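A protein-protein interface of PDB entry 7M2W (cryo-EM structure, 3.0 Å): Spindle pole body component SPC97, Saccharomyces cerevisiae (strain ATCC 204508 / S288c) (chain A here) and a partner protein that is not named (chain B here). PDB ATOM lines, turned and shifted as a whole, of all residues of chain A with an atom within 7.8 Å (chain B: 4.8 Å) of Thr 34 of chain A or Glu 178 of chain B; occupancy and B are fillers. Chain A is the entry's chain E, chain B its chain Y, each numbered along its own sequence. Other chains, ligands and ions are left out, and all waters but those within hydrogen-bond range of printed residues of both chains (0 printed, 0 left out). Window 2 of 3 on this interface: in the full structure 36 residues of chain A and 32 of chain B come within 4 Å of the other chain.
O of Thr 34 of chain A lies within hydrogen-bond range of ND2 of Asn 185 of chain B, at 3.0 Å.
ND2 of Asn 35 of chain A lies within hydrogen-bond range of OD2 of Asp 181 of chain B (3.2 Å).
The side-chain hydroxyl (OG1) of Thr 34 of chain A sits at hydrogen-bond distance from the side-chain amide oxygen (OD1) of Asn 35 of chain A, 2.6 Å away.
OE2 of Glu 82 of chain A lies within hydrogen-bond range of OG of Ser 84 of chain A (2.5 Å).
The side-chain carboxylate (OD1) of Asp 181 of chain B is in salt-bridge range of the side-chain amino group (NZ) of Lys 177 of chain B, 2.8 Å away.
O of Glu 178 of chain B is in hydrogen-bond range of OG1 of Thr 182 of chain B (2.6 Å).
The backbone carbonyl oxygen (O) of Asp 181 of chain B lies close to the side-chain amide oxygen (OD1) of Asn 185 of chain B.
Among the printed residues, merely in contact across the chains: Thr 34 of chain A with Glu 178 of chain B, Thr 34 of chain A with Asp 181 of chain B, Thr 34 of chain A with Thr 182 of chain B, Glu 82 of chain A with Leu 175 of chain B, Glu 82 of chain A with Glu 178 of chain B and Ser 84 of chain A with Glu 174 of chain B.
Of the printed residues of chain B, Thr 34 of chain A touches Glu 178 (3.4 Å), Asp 181 (3.8 Å), Thr 182 (2.8 Å) and Asn 185 (3.0 Å).
Lys 37 of chain A touches none of the printed residues of chain B.
Printed residues of chain B within 4 Å of Glu 82 of chain A: Leu 175 and Glu 178.
Of the printed residues of chain A, Leu 175 of chain B touches Glu 82 (3.4 Å).
Of the printed residues of chain A, Glu 178 of chain B touches Thr 34 (3.4 Å) and Glu 82 (3.97 Å).
Lys 179 of chain B touches none of the printed residues of chain A.
Of the printed residues of chain A, Thr 182 of chain B touches Thr 34 (2.8 Å).
The nearest printed residue of chain A that does not touch Glu 174 of chain B is Glu 82 of chain A (5.3 Å).
Of the 17 printed residues of chain A, 4 touch a printed residue of chain B.
Hydrophobic or aromatic side chains of chain B that line the printed part of chain A: Leu 175.
Along chain B the printed residues that touch a printed residue of chain A span positions 174 to 185.
Among the printed residues, 8 pairs touch across the chains.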
ATOM      1  N   VAL A   6       1.890  24.660 -35.669  1.00  0.00           N
ATOM      2  CA  VAL A   6       2.484  25.506 -34.644  1.00  0.00           C
ATOM      3  C   VAL A   6       2.900  26.818 -35.288  1.00  0.00           C
ATOM      4  O   VAL A   6       3.313  26.858 -36.452  1.00  0.00           O
ATOM      5  CB  VAL A   6       3.690  24.836 -33.955  1.00  0.00           C
ATOM      6  CG1 VAL A   6       3.226  23.718 -33.039  1.00  0.00           C
ATOM      7  CG2 VAL A   6       4.657  24.310 -34.985  1.00  0.00           C
ATOM      8  N   GLN A  29      14.419  27.932 -33.788  1.00  0.00           N
ATOM      9  CA  GLN A  29      13.276  27.259 -34.373  1.00  0.00           C
ATOM     10  C   GLN A  29      12.476  26.538 -33.289  1.00  0.00           C
ATOM     11  O   GLN A  29      12.945  26.384 -32.160  1.00  0.00           O
ATOM     12  CB  GLN A  29      13.747  26.276 -35.437  1.00  0.00           C
ATOM     13  CG  GLN A  29      14.101  24.909 -34.897  1.00  0.00           C
ATOM     14  CD  GLN A  29      15.574  24.772 -34.590  1.00  0.00           C
ATOM     15  OE1 GLN A  29      16.322  25.745 -34.642  1.00  0.00           O
ATOM     16  NE2 GLN A  29      16.000  23.558 -34.270  1.00  0.00           N
ATOM     17  N   PRO A  30      11.260  26.088 -33.606  1.00  0.00           N
ATOM     18  CA  PRO A  30      10.479  25.350 -32.608  1.00  0.00           C
ATOM     19  C   PRO A  30      11.075  23.977 -32.343  1.00  0.00           C
ATOM     20  O   PRO A  30      11.349  23.210 -33.265  1.00  0.00           O
ATOM     21  CB  PRO A  30       9.092  25.248 -33.251  1.00  0.00           C
ATOM     22  CG  PRO A  30       9.062  26.324 -34.270  1.00  0.00           C
ATOM     23  CD  PRO A  30      10.452  26.393 -34.796  1.00  0.00           C
ATOM     24  N   LEU A  31      11.268  23.671 -31.066  1.00  0.00           N
ATOM     25  CA  LEU A  31      11.868  22.413 -30.655  1.00  0.00           C
ATOM     26  C   LEU A  31      10.870  21.271 -30.783  1.00  0.00           C
ATOM     27  O   LEU A  31       9.672  21.438 -30.548  1.00  0.00           O
ATOM     28  CB  LEU A  31      12.372  22.499 -29.215  1.00  0.00           C
ATOM     29  CG  LEU A  31      13.394  23.596 -28.926  1.00  0.00           C
ATOM     30  CD1 LEU A  31      13.923  23.468 -27.512  1.00  0.00           C
ATOM     31  CD2 LEU A  31      14.526  23.546 -29.931  1.00  0.00           C
ATOM     32  N   TRP A  32      11.379  20.098 -31.168  1.00  0.00           N
ATOM     33  CA  TRP A  32      10.532  18.917 -31.263  1.00  0.00           C
ATOM     34  C   TRP A  32       9.906  18.549 -29.927  1.00  0.00           C
ATOM     35  O   TRP A  32       8.813  17.975 -29.901  1.00  0.00           O
ATOM     36  CB  TRP A  32      11.333  17.724 -31.780  1.00  0.00           C
ATOM     37  CG  TRP A  32      11.475  17.672 -33.262  1.00  0.00           C
ATOM     38  CD1 TRP A  32      12.518  18.143 -34.002  1.00  0.00           C
ATOM     39  CD2 TRP A  32      10.547  17.108 -34.192  1.00  0.00           C
ATOM     40  NE1 TRP A  32      12.298  17.906 -35.335  1.00  0.00           N
ATOM     41  CE2 TRP A  32      11.092  17.276 -35.479  1.00  0.00           C
ATOM     42  CE3 TRP A  32       9.307  16.480 -34.062  1.00  0.00           C
ATOM     43  CZ2 TRP A  32      10.441  16.838 -36.626  1.00  0.00           C
ATOM     44  CZ3 TRP A  32       8.665  16.044 -35.200  1.00  0.00           C
ATOM     45  CH2 TRP A  32       9.232  16.224 -36.465  1.00  0.00           C
ATOM     46  N   SER A  33      10.571  18.867 -28.819  1.00  0.00           N
ATOM     47  CA  SER A  33      10.075  18.491 -27.505  1.00  0.00           C
ATOM     48  C   SER A  33       8.845  19.281 -27.084  1.00  0.00           C
ATOM     49  O   SER A  33       8.081  18.803 -26.241  1.00  0.00           O
ATOM     50  CB  SER A  33      11.179  18.669 -26.462  1.00  0.00           C
ATOM     51  OG  SER A  33      12.338  17.942 -26.830  1.00  0.00           O
ATOM     52  N   THR A  34       8.633  20.471 -27.644  1.00  0.00           N
ATOM     53  CA  THR A  34       7.515  21.299 -27.213  1.00  0.00           C
ATOM     54  C   THR A  34       6.615  21.711 -28.372  1.00  0.00           C
ATOM     55  O   THR A  34       5.430  21.989 -28.166  1.00  0.00           O
ATOM     56  CB  THR A  34       8.018  22.551 -26.491  1.00  0.00           C
ATOM     57  OG1 THR A  34       8.693  23.402 -27.423  1.00  0.00           O
ATOM     58  CG2 THR A  34       8.975  22.180 -25.372  1.00  0.00           C
ATOM     59  N   ASN A  35       7.153  21.756 -29.588  1.00  0.00           N
ATOM     60  CA  ASN A  35       6.408  22.224 -30.760  1.00  0.00           C
ATOM     61  C   ASN A  35       6.745  21.367 -31.972  1.00  0.00           C
ATOM     62  O   ASN A  35       7.387  21.828 -32.922  1.00  0.00           O
ATOM     63  CB  ASN A  35       6.706  23.697 -31.046  1.00  0.00           C
ATOM     64  CG  ASN A  35       6.319  24.608 -29.900  1.00  0.00           C
ATOM     65  OD1 ASN A  35       6.966  24.621 -28.855  1.00  0.00           O
ATOM     66  ND2 ASN A  35       5.259  25.382 -30.094  1.00  0.00           N
ATOM     67  N   PRO A  36       6.326  20.102 -31.975  1.00  0.00           N
ATOM     68  CA  PRO A  36       6.594  19.253 -33.139  1.00  0.00           C
ATOM     69  C   PRO A  36       5.721  19.638 -34.321  1.00  0.00           C
ATOM     70  O   PRO A  36       4.532  19.922 -34.172  1.00  0.00           O
ATOM     71  CB  PRO A  36       6.264  17.845 -32.635  1.00  0.00           C
ATOM     72  CG  PRO A  36       5.268  18.060 -31.569  1.00  0.00           C
ATOM     73  CD  PRO A  36       5.574  19.385 -30.930  1.00  0.00           C
ATOM     74  N   LYS A  37       6.327  19.652 -35.507  1.00  0.00           N
ATOM     75  CA  LYS A  37       5.616  19.950 -36.740  1.00  0.00           C
ATOM     76  C   LYS A  37       5.293  18.707 -37.548  1.00  0.00           C
ATOM     77  O   LYS A  37       4.913  18.825 -38.715  1.00  0.00           O
ATOM     78  CB  LYS A  37       6.430  20.908 -37.611  1.00  0.00           C
ATOM     79  CG  LYS A  37       6.619  22.287 -37.027  1.00  0.00           C
ATOM     80  CD  LYS A  37       6.522  23.340 -38.111  1.00  0.00           C
ATOM     81  CE  LYS A  37       7.505  24.463 -37.878  1.00  0.00           C
ATOM     82  NZ  LYS A  37       7.491  25.430 -39.002  1.00  0.00           N
ATOM     83  N   GLU A  71      17.915  19.348 -35.121  1.00  0.00           N
ATOM     84  CA  GLU A  71      17.311  18.107 -34.672  1.00  0.00           C
ATOM     85  C   GLU A  71      16.458  17.498 -35.772  1.00  0.00           C
ATOM     86  O   GLU A  71      15.638  18.174 -36.394  1.00  0.00           O
ATOM     87  CB  GLU A  71      16.463  18.340 -33.425  1.00  0.00           C
ATOM     88  CG  GLU A  71      15.544  19.529 -33.546  1.00  0.00           C
ATOM     89  CD  GLU A  71      14.833  19.840 -32.256  1.00  0.00           C
ATOM     90  OE1 GLU A  71      14.975  19.059 -31.296  1.00  0.00           O
ATOM     91  OE2 GLU A  71      14.142  20.875 -32.200  1.00  0.00           O
ATOM     92  N   ARG A  76      16.554  13.920 -31.530  1.00  0.00           N
ATOM     93  CA  ARG A  76      16.105  15.205 -31.022  1.00  0.00           C
ATOM     94  C   ARG A  76      17.027  15.674 -29.908  1.00  0.00           C
ATOM     95  O   ARG A  76      17.854  14.914 -29.399  1.00  0.00           O
ATOM     96  CB  ARG A  76      14.664  15.106 -30.522  1.00  0.00           C
ATOM     97  CG  ARG A  76      13.785  14.336 -31.479  1.00  0.00           C
ATOM     98  CD  ARG A  76      12.338  14.337 -31.061  1.00  0.00           C
ATOM     99  NE  ARG A  76      11.500  13.788 -32.119  1.00  0.00           N
ATOM    100  CZ  ARG A  76      10.187  13.959 -32.195  1.00  0.00           C
ATOM    101  NH1 ARG A  76       9.551  14.667 -31.273  1.00  0.00           N
ATOM    102  NH2 ARG A  76       9.506  13.424 -33.199  1.00  0.00           N
ATOM    103  N   ASN A  79      16.694  16.654 -23.139  1.00  0.00           N
ATOM    104  CA  ASN A  79      15.593  17.258 -22.398  1.00  0.00           C
ATOM    105  C   ASN A  79      16.028  18.522 -21.669  1.00  0.00           C
ATOM    106  O   ASN A  79      15.201  19.400 -21.399  1.00  0.00           O
ATOM    107  CB  ASN A  79      15.011  16.248 -21.408  1.00  0.00           C
ATOM    108  CG  ASN A  79      14.299  15.103 -22.098  1.00  0.00           C
ATOM    109  OD1 ASN A  79      13.726  15.274 -23.173  1.00  0.00           O
ATOM    110  ND2 ASN A  79      14.331  13.927 -21.483  1.00  0.00           N
ATOM    111  N   TYR A  81      18.171  20.690 -22.906  1.00  0.00           N
ATOM    112  CA  TYR A  81      18.639  21.676 -23.869  1.00  0.00           C
ATOM    113  C   TYR A  81      17.724  22.893 -23.865  1.00  0.00           C
ATOM    114  O   TYR A  81      16.517  22.778 -24.096  1.00  0.00           O
ATOM    115  CB  TYR A  81      18.700  21.066 -25.266  1.00  0.00           C
ATOM    116  CG  TYR A  81      19.209  22.010 -26.330  1.00  0.00           C
ATOM    117  CD1 TYR A  81      20.565  22.230 -26.499  1.00  0.00           C
ATOM    118  CD2 TYR A  81      18.330  22.673 -27.174  1.00  0.00           C
ATOM    119  CE1 TYR A  81      21.031  23.088 -27.473  1.00  0.00           C
ATOM    120  CE2 TYR A  81      18.788  23.531 -28.149  1.00  0.00           C
ATOM    121  CZ  TYR A  81      20.139  23.735 -28.294  1.00  0.00           C
ATOM    122  OH  TYR A  81      20.604  24.590 -29.264  1.00  0.00           O
ATOM    123  N   GLU A  82      18.304  24.061 -23.608  1.00  0.00           N
ATOM    124  CA  GLU A  82      17.570  25.323 -23.617  1.00  0.00           C
ATOM    125  C   GLU A  82      18.228  26.228 -24.647  1.00  0.00           C
ATOM    126  O   GLU A  82      19.324  26.761 -24.400  1.00  0.00           O
ATOM    127  CB  GLU A  82      17.563  25.971 -22.238  1.00  0.00           C
ATOM    128  CG  GLU A  82      16.851  27.309 -22.185  1.00  0.00           C
ATOM    129  CD  GLU A  82      15.412  27.225 -22.658  1.00  0.00           C
ATOM    130  OE1 GLU A  82      14.701  26.286 -22.240  1.00  0.00           O
ATOM    131  OE2 GLU A  82      14.990  28.098 -23.444  1.00  0.00           O
ATOM    132  N   PRO A  83      17.600  26.429 -25.805  1.00  0.00           N
ATOM    133  CA  PRO A  83      18.273  27.164 -26.887  1.00  0.00           C
ATOM    134  C   PRO A  83      18.506  28.630 -26.580  1.00  0.00           C
ATOM    135  O   PRO A  83      19.478  29.205 -27.086  1.00  0.00           O
ATOM    136  CB  PRO A  83      17.314  26.987 -28.070  1.00  0.00           C
ATOM    137  CG  PRO A  83      15.977  26.824 -27.433  1.00  0.00           C
ATOM    138  CD  PRO A  83      16.220  26.057 -26.162  1.00  0.00           C
ATOM    139  N   SER A  84      17.656  29.256 -25.773  1.00  0.00           N
ATOM    140  CA  SER A  84      17.833  30.656 -25.412  1.00  0.00           C
ATOM    141  C   SER A  84      18.942  30.873 -24.391  1.00  0.00           C
ATOM    142  O   SER A  84      19.118  32.004 -23.927  1.00  0.00           O
ATOM    143  CB  SER A  84      16.518  31.227 -24.875  1.00  0.00           C
ATOM    144  OG  SER A  84      15.892  30.321 -23.984  1.00  0.00           O
ATOM    145  N   GLU B 174       9.301  33.125 -22.438  1.00  0.00           N
ATOM    146  CA  GLU B 174       9.589  32.023 -23.361  1.00  0.00           C
ATOM    147  C   GLU B 174       9.437  30.659 -22.674  1.00  0.00           C
ATOM    148  O   GLU B 174       8.738  29.797 -23.199  1.00  0.00           O
ATOM    149  CB  GLU B 174      10.996  32.175 -23.957  1.00  0.00           C
ATOM    150  CG  GLU B 174      11.055  33.305 -24.997  1.00  0.00           C
ATOM    151  CD  GLU B 174      12.487  33.670 -25.412  1.00  0.00           C
ATOM    152  OE1 GLU B 174      13.381  32.801 -25.381  1.00  0.00           O
ATOM    153  OE2 GLU B 174      12.713  34.825 -25.827  1.00  0.00           O
ATOM    154  N   LEU B 175      10.002  30.471 -21.476  1.00  0.00           N
ATOM    155  CA  LEU B 175       9.837  29.244 -20.696  1.00  0.00           C
ATOM    156  C   LEU B 175       8.374  29.003 -20.310  1.00  0.00           C
ATOM    157  O   LEU B 175       7.903  27.879 -20.444  1.00  0.00           O
ATOM    158  CB  LEU B 175      10.708  29.285 -19.430  1.00  0.00           C
ATOM    159  CG  LEU B 175      12.211  29.056 -19.658  1.00  0.00           C
ATOM    160  CD1 LEU B 175      12.974  29.339 -18.365  1.00  0.00           C
ATOM    161  CD2 LEU B 175      12.502  27.606 -20.051  1.00  0.00           C
ATOM    162  N   ARG B 176       7.630  30.029 -19.875  1.00  0.00           N
ATOM    163  CA  ARG B 176       6.197  29.911 -19.542  1.00  0.00           C
ATOM    164  C   ARG B 176       5.366  29.486 -20.758  1.00  0.00           C
ATOM    165  O   ARG B 176       4.602  28.527 -20.667  1.00  0.00           O
ATOM    166  CB  ARG B 176       5.677  31.224 -18.925  1.00  0.00           C
ATOM    167  CG  ARG B 176       6.150  31.392 -17.472  1.00  0.00           C
ATOM    168  CD  ARG B 176       5.686  32.725 -16.870  1.00  0.00           C
ATOM    169  NE  ARG B 176       6.168  32.901 -15.483  1.00  0.00           N
ATOM    170  CZ  ARG B 176       5.678  32.354 -14.387  1.00  0.00           C
ATOM    171  NH1 ARG B 176       4.657  31.551 -14.408  1.00  0.00           N
ATOM    172  NH2 ARG B 176       6.210  32.595 -13.228  1.00  0.00           N
ATOM    173  N   LYS B 177       5.566  30.115 -21.920  1.00  0.00           N
ATOM    174  CA  LYS B 177       4.905  29.726 -23.179  1.00  0.00           C
ATOM    175  C   LYS B 177       5.280  28.302 -23.600  1.00  0.00           C
ATOM    176  O   LYS B 177       4.408  27.482 -23.864  1.00  0.00           O
ATOM    177  CB  LYS B 177       5.239  30.764 -24.267  1.00  0.00           C
ATOM    178  CG  LYS B 177       4.564  30.513 -25.626  1.00  0.00           C
ATOM    179  CD  LYS B 177       3.031  30.466 -25.542  1.00  0.00           C
ATOM    180  CE  LYS B 177       2.346  30.502 -26.915  1.00  0.00           C
ATOM    181  NZ  LYS B 177       2.589  29.283 -27.723  1.00  0.00           N
ATOM    182  N   GLU B 178       6.568  27.974 -23.591  1.00  0.00           N
ATOM    183  CA  GLU B 178       7.077  26.652 -23.963  1.00  0.00           C
ATOM    184  C   GLU B 178       6.570  25.545 -23.023  1.00  0.00           C
ATOM    185  O   GLU B 178       6.165  24.477 -23.483  1.00  0.00           O
ATOM    186  CB  GLU B 178       8.609  26.733 -23.992  1.00  0.00           C
ATOM    187  CG  GLU B 178       9.270  25.421 -24.412  1.00  0.00           C
ATOM    188  CD  GLU B 178      10.772  25.594 -24.689  1.00  0.00           C
ATOM    189  OE1 GLU B 178      11.154  26.535 -25.415  1.00  0.00           O
ATOM    190  OE2 GLU B 178      11.574  24.789 -24.172  1.00  0.00           O
ATOM    191  N   LYS B 179       6.512  25.813 -21.713  1.00  0.00           N
ATOM    192  CA  LYS B 179       5.869  24.957 -20.710  1.00  0.00           C
ATOM    193  C   LYS B 179       4.395  24.750 -21.045  1.00  0.00           C
ATOM    194  O   LYS B 179       3.971  23.605 -21.122  1.00  0.00           O
ATOM    195  CB  LYS B 179       6.069  25.574 -19.312  1.00  0.00           C
ATOM    196  CG  LYS B 179       5.302  24.848 -18.197  1.00  0.00           C
ATOM    197  CD  LYS B 179       5.427  25.587 -16.859  1.00  0.00           C
ATOM    198  CE  LYS B 179       4.452  24.990 -15.836  1.00  0.00           C
ATOM    199  NZ  LYS B 179       4.400  25.783 -14.585  1.00  0.00           N
ATOM    200  N   ASN B 180       3.626  25.811 -21.287  1.00  0.00           N
ATOM    201  CA  ASN B 180       2.199  25.698 -21.610  1.00  0.00           C
ATOM    202  C   ASN B 180       1.954  24.895 -22.899  1.00  0.00           C
ATOM    203  O   ASN B 180       1.099  24.014 -22.915  1.00  0.00           O
ATOM    204  CB  ASN B 180       1.563  27.097 -21.683  1.00  0.00           C
ATOM    205  CG  ASN B 180       1.462  27.799 -20.338  1.00  0.00           C
ATOM    206  OD1 ASN B 180       1.684  27.229 -19.282  1.00  0.00           O
ATOM    207  ND2 ASN B 180       1.085  29.052 -20.335  1.00  0.00           N
ATOM    208  N   ASP B 181       2.748  25.111 -23.948  1.00  0.00           N
ATOM    209  CA  ASP B 181       2.704  24.293 -25.168  1.00  0.00           C
ATOM    210  C   ASP B 181       2.998  22.817 -24.864  1.00  0.00           C
ATOM    211  O   ASP B 181       2.247  21.922 -25.249  1.00  0.00           O
ATOM    212  CB  ASP B 181       3.721  24.814 -26.196  1.00  0.00           C
ATOM    213  CG  ASP B 181       3.446  26.232 -26.705  1.00  0.00           C
ATOM    214  OD1 ASP B 181       2.312  26.742 -26.568  1.00  0.00           O
ATOM    215  OD2 ASP B 181       4.353  26.814 -27.336  1.00  0.00           O
ATOM    216  N   THR B 182       4.055  22.557 -24.098  1.00  0.00           N
ATOM    217  CA  THR B 182       4.435  21.202 -23.687  1.00  0.00           C
ATOM    218  C   THR B 182       3.346  20.542 -22.838  1.00  0.00           C
ATOM    219  O   THR B 182       3.058  19.364 -23.015  1.00  0.00           O
ATOM    220  CB  THR B 182       5.769  21.234 -22.936  1.00  0.00           C
ATOM    221  OG1 THR B 182       6.725  21.910 -23.709  1.00  0.00           O
ATOM    222  CG2 THR B 182       6.339  19.845 -22.683  1.00  0.00           C
ATOM    223  N   ASN B 185       0.566  19.431 -25.157  1.00  0.00           N
ATOM    224  CA  ASN B 185       0.969  18.123 -25.686  1.00  0.00           C
ATOM    225  C   ASN B 185       0.744  17.018 -24.642  1.00  0.00           C
ATOM    226  O   ASN B 185       0.139  15.999 -24.955  1.00  0.00           O
ATOM    227  CB  ASN B 185       2.439  18.120 -26.148  1.00  0.00           C
ATOM    228  CG  ASN B 185       2.831  19.240 -27.090  1.00  0.00           C
ATOM    229  OD1 ASN B 185       2.025  19.850 -27.772  1.00  0.00           O
ATOM    230  ND2 ASN B 185       4.105  19.533 -27.147  1.00  0.00           N
